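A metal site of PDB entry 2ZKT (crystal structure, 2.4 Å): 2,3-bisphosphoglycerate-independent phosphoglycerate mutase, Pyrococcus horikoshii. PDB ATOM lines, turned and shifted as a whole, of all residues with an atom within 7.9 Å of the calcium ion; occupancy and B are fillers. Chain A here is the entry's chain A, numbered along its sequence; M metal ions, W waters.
N of Asp 373 lies within hydrogen-bond range of O of Gly 44, 3.2 Å away. The side-chain hydroxyl of Thr 372 sits close to the backbone carbonyl oxygen of Ile 43, 3.2 Å away. The side-chain hydroxyl (OG1) of Thr 372 sits close to the backbone carbonyl oxygen (O) of Gly 44, 2.9 Å away. The side-chain hydroxyl (OG1) of Thr 375 lies within hydrogen-bond range of the side-chain carboxylate (OD1) of Asp 373 (2.6 Å). The side-chain carboxylate (OE2) of Glu 42 is in salt-bridge range of the side-chain amino group (NZ) of Lys 376.
Within 4 Å of the calcium ion: Glu 42, Thr 372 and Asp 373. The nearest printed residue that does not touch the calcium ion is Thr 375 (4.1 Å).
The calcium ion is bound by water W1 (2.3 Å), O of Asp 373 (2.4 Å), O of Glu 42 (2.4 Å), OG1 of Thr 372 (2.5 Å) and water W2 (2.5 Å).
Water W1 lies within hydrogen-bond range of O of Thr 375, NZ of Lys 376 and OE2 of Glu 42.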
ATOM      1  N   LYS A  39      14.402  26.897   7.109  1.00  0.00           N
ATOM      2  CA  LYS A  39      15.091  25.624   6.895  1.00  0.00           C
ATOM      3  C   LYS A  39      15.578  25.072   8.237  1.00  0.00           C
ATOM      4  O   LYS A  39      15.370  23.902   8.562  1.00  0.00           O
ATOM      5  CB  LYS A  39      16.273  25.837   5.939  1.00  0.00           C
ATOM      6  CG  LYS A  39      17.135  24.610   5.693  1.00  0.00           C
ATOM      7  CD  LYS A  39      18.457  25.054   5.065  1.00  0.00           C
ATOM      8  CE  LYS A  39      19.464  23.916   4.986  1.00  0.00           C
ATOM      9  NZ  LYS A  39      20.816  24.425   4.564  1.00  0.00           N
ATOM     10  N   LEU A  40      16.229  25.931   9.037  1.00  0.00           N
ATOM     11  CA  LEU A  40      16.738  25.518  10.341  1.00  0.00           C
ATOM     12  C   LEU A  40      15.596  25.109  11.279  1.00  0.00           C
ATOM     13  O   LEU A  40      15.726  24.171  12.069  1.00  0.00           O
ATOM     14  CB  LEU A  40      17.582  26.645  10.962  1.00  0.00           C
ATOM     15  CG  LEU A  40      18.935  26.897  10.282  1.00  0.00           C
ATOM     16  CD1 LEU A  40      19.550  28.193  10.801  1.00  0.00           C
ATOM     17  CD2 LEU A  40      19.874  25.716  10.544  1.00  0.00           C
ATOM     18  N   ALA A  41      14.468  25.823  11.196  1.00  0.00           N
ATOM     19  CA  ALA A  41      13.318  25.499  12.036  1.00  0.00           C
ATOM     20  C   ALA A  41      12.854  24.092  11.648  1.00  0.00           C
ATOM     21  O   ALA A  41      12.580  23.237  12.500  1.00  0.00           O
ATOM     22  CB  ALA A  41      12.195  26.496  11.802  1.00  0.00           C
ATOM     23  N   GLU A  42      12.806  23.843  10.346  1.00  0.00           N
ATOM     24  CA  GLU A  42      12.370  22.563   9.805  1.00  0.00           C
ATOM     25  C   GLU A  42      13.263  21.399  10.281  1.00  0.00           C
ATOM     26  O   GLU A  42      12.752  20.347  10.653  1.00  0.00           O
ATOM     27  CB  GLU A  42      12.325  22.643   8.278  1.00  0.00           C
ATOM     28  CG  GLU A  42      11.375  21.668   7.584  1.00  0.00           C
ATOM     29  CD  GLU A  42      11.921  20.254   7.490  1.00  0.00           C
ATOM     30  OE1 GLU A  42      13.149  20.097   7.288  1.00  0.00           O
ATOM     31  OE2 GLU A  42      11.122  19.287   7.596  1.00  0.00           O
ATOM     32  N   ILE A  43      14.579  21.567  10.282  1.00  0.00           N
ATOM     33  CA  ILE A  43      15.466  20.487  10.743  1.00  0.00           C
ATOM     34  C   ILE A  43      15.717  20.558  12.256  1.00  0.00           C
ATOM     35  O   ILE A  43      16.221  19.605  12.858  1.00  0.00           O
ATOM     36  CB  ILE A  43      16.852  20.520  10.057  1.00  0.00           C
ATOM     37  CG1 ILE A  43      17.420  21.944  10.107  1.00  0.00           C
ATOM     38  CG2 ILE A  43      16.758  19.969   8.652  1.00  0.00           C
ATOM     39  CD1 ILE A  43      18.750  22.105   9.413  1.00  0.00           C
ATOM     40  N   GLY A  44      15.369  21.677  12.875  1.00  0.00           N
ATOM     41  CA  GLY A  44      15.592  21.835  14.299  1.00  0.00           C
ATOM     42  C   GLY A  44      14.363  21.679  15.176  1.00  0.00           C
ATOM     43  O   GLY A  44      13.479  20.846  14.913  1.00  0.00           O
ATOM     44  N   ILE A  45      14.325  22.490  16.235  1.00  0.00           N
ATOM     45  CA  ILE A  45      13.229  22.474  17.195  1.00  0.00           C
ATOM     46  C   ILE A  45      12.958  23.926  17.610  1.00  0.00           C
ATOM     47  O   ILE A  45      13.875  24.759  17.669  1.00  0.00           O
ATOM     48  CB  ILE A  45      13.606  21.621  18.431  1.00  0.00           C
ATOM     49  CG1 ILE A  45      12.402  21.462  19.366  1.00  0.00           C
ATOM     50  CG2 ILE A  45      14.774  22.263  19.185  1.00  0.00           C
ATOM     51  CD1 ILE A  45      12.662  20.442  20.509  1.00  0.00           C
ATOM     52  N   ARG A 371      16.372  16.889  18.829  1.00  0.00           N
ATOM     53  CA  ARG A 371      15.226  16.037  18.513  1.00  0.00           C
ATOM     54  C   ARG A 371      14.231  16.913  17.734  1.00  0.00           C
ATOM     55  O   ARG A 371      13.315  17.509  18.292  1.00  0.00           O
ATOM     56  CB  ARG A 371      14.610  15.493  19.828  1.00  0.00           C
ATOM     57  CG  ARG A 371      15.672  14.830  20.708  1.00  0.00           C
ATOM     58  CD  ARG A 371      15.121  13.931  21.804  1.00  0.00           C
ATOM     59  NE  ARG A 371      14.459  14.680  22.862  1.00  0.00           N
ATOM     60  CZ  ARG A 371      14.403  14.297  24.138  1.00  0.00           C
ATOM     61  NH1 ARG A 371      14.980  13.161  24.525  1.00  0.00           N
ATOM     62  NH2 ARG A 371      13.747  15.037  25.021  1.00  0.00           N
ATOM     63  N   THR A 372      14.446  16.988  16.421  1.00  0.00           N
ATOM     64  CA  THR A 372      13.610  17.827  15.554  1.00  0.00           C
ATOM     65  C   THR A 372      12.097  17.623  15.733  1.00  0.00           C
ATOM     66  O   THR A 372      11.614  16.490  15.723  1.00  0.00           O
ATOM     67  CB  THR A 372      13.991  17.613  14.066  1.00  0.00           C
ATOM     68  OG1 THR A 372      13.248  18.514  13.249  1.00  0.00           O
ATOM     69  CG2 THR A 372      13.690  16.176  13.621  1.00  0.00           C
ATOM     70  N   ASP A 373      11.354  18.721  15.909  1.00  0.00           N
ATOM     71  CA  ASP A 373       9.905  18.636  16.084  1.00  0.00           C
ATOM     72  C   ASP A 373       9.282  18.685  14.709  1.00  0.00           C
ATOM     73  O   ASP A 373       9.947  18.349  13.735  1.00  0.00           O
ATOM     74  CB  ASP A 373       9.380  19.785  16.977  1.00  0.00           C
ATOM     75  CG  ASP A 373       9.831  21.161  16.494  1.00  0.00           C
ATOM     76  OD1 ASP A 373      10.235  21.301  15.323  1.00  0.00           O
ATOM     77  OD2 ASP A 373       9.758  22.122  17.293  1.00  0.00           O
ATOM     78  N   ASP A 374       8.024  19.110  14.595  1.00  0.00           N
ATOM     79  CA  ASP A 374       7.386  19.159  13.274  1.00  0.00           C
ATOM     80  C   ASP A 374       7.011  20.554  12.777  1.00  0.00           C
ATOM     81  O   ASP A 374       6.045  20.734  12.025  1.00  0.00           O
ATOM     82  CB  ASP A 374       6.168  18.209  13.239  1.00  0.00           C
ATOM     83  CG  ASP A 374       5.214  18.431  14.395  1.00  0.00           C
ATOM     84  OD1 ASP A 374       5.676  18.545  15.556  1.00  0.00           O
ATOM     85  OD2 ASP A 374       3.981  18.482  14.147  1.00  0.00           O
ATOM     86  N   THR A 375       7.764  21.559  13.216  1.00  0.00           N
ATOM     87  CA  THR A 375       7.563  22.946  12.790  1.00  0.00           C
ATOM     88  C   THR A 375       8.237  23.075  11.410  1.00  0.00           C
ATOM     89  O   THR A 375       9.209  22.362  11.124  1.00  0.00           O
ATOM     90  CB  THR A 375       8.206  23.937  13.779  1.00  0.00           C
ATOM     91  OG1 THR A 375       9.545  23.508  14.078  1.00  0.00           O
ATOM     92  CG2 THR A 375       7.404  24.027  15.073  1.00  0.00           C
ATOM     93  N   LYS A 376       7.739  23.977  10.566  1.00  0.00           N
ATOM     94  CA  LYS A 376       8.279  24.158   9.221  1.00  0.00           C
ATOM     95  C   LYS A 376       8.797  25.569   8.926  1.00  0.00           C
ATOM     96  O   LYS A 376       9.443  25.796   7.898  1.00  0.00           O
ATOM     97  CB  LYS A 376       7.207  23.801   8.164  1.00  0.00           C
ATOM     98  CG  LYS A 376       6.669  22.375   8.240  1.00  0.00           C
ATOM     99  CD  LYS A 376       7.746  21.356   7.873  1.00  0.00           C
ATOM    100  CE  LYS A 376       7.203  19.926   7.858  1.00  0.00           C
ATOM    101  NZ  LYS A 376       8.263  18.940   7.465  1.00  0.00           N
HETATM  102 CA    CA M   1      11.255  18.911  11.830  1.00  0.00          CA
HETATM  103  O   HOH W   1       9.414  19.485  10.625  1.00  0.00           O
HETATM  104  O   HOH W   2      11.228  21.091  13.009  1.00  0.00           O
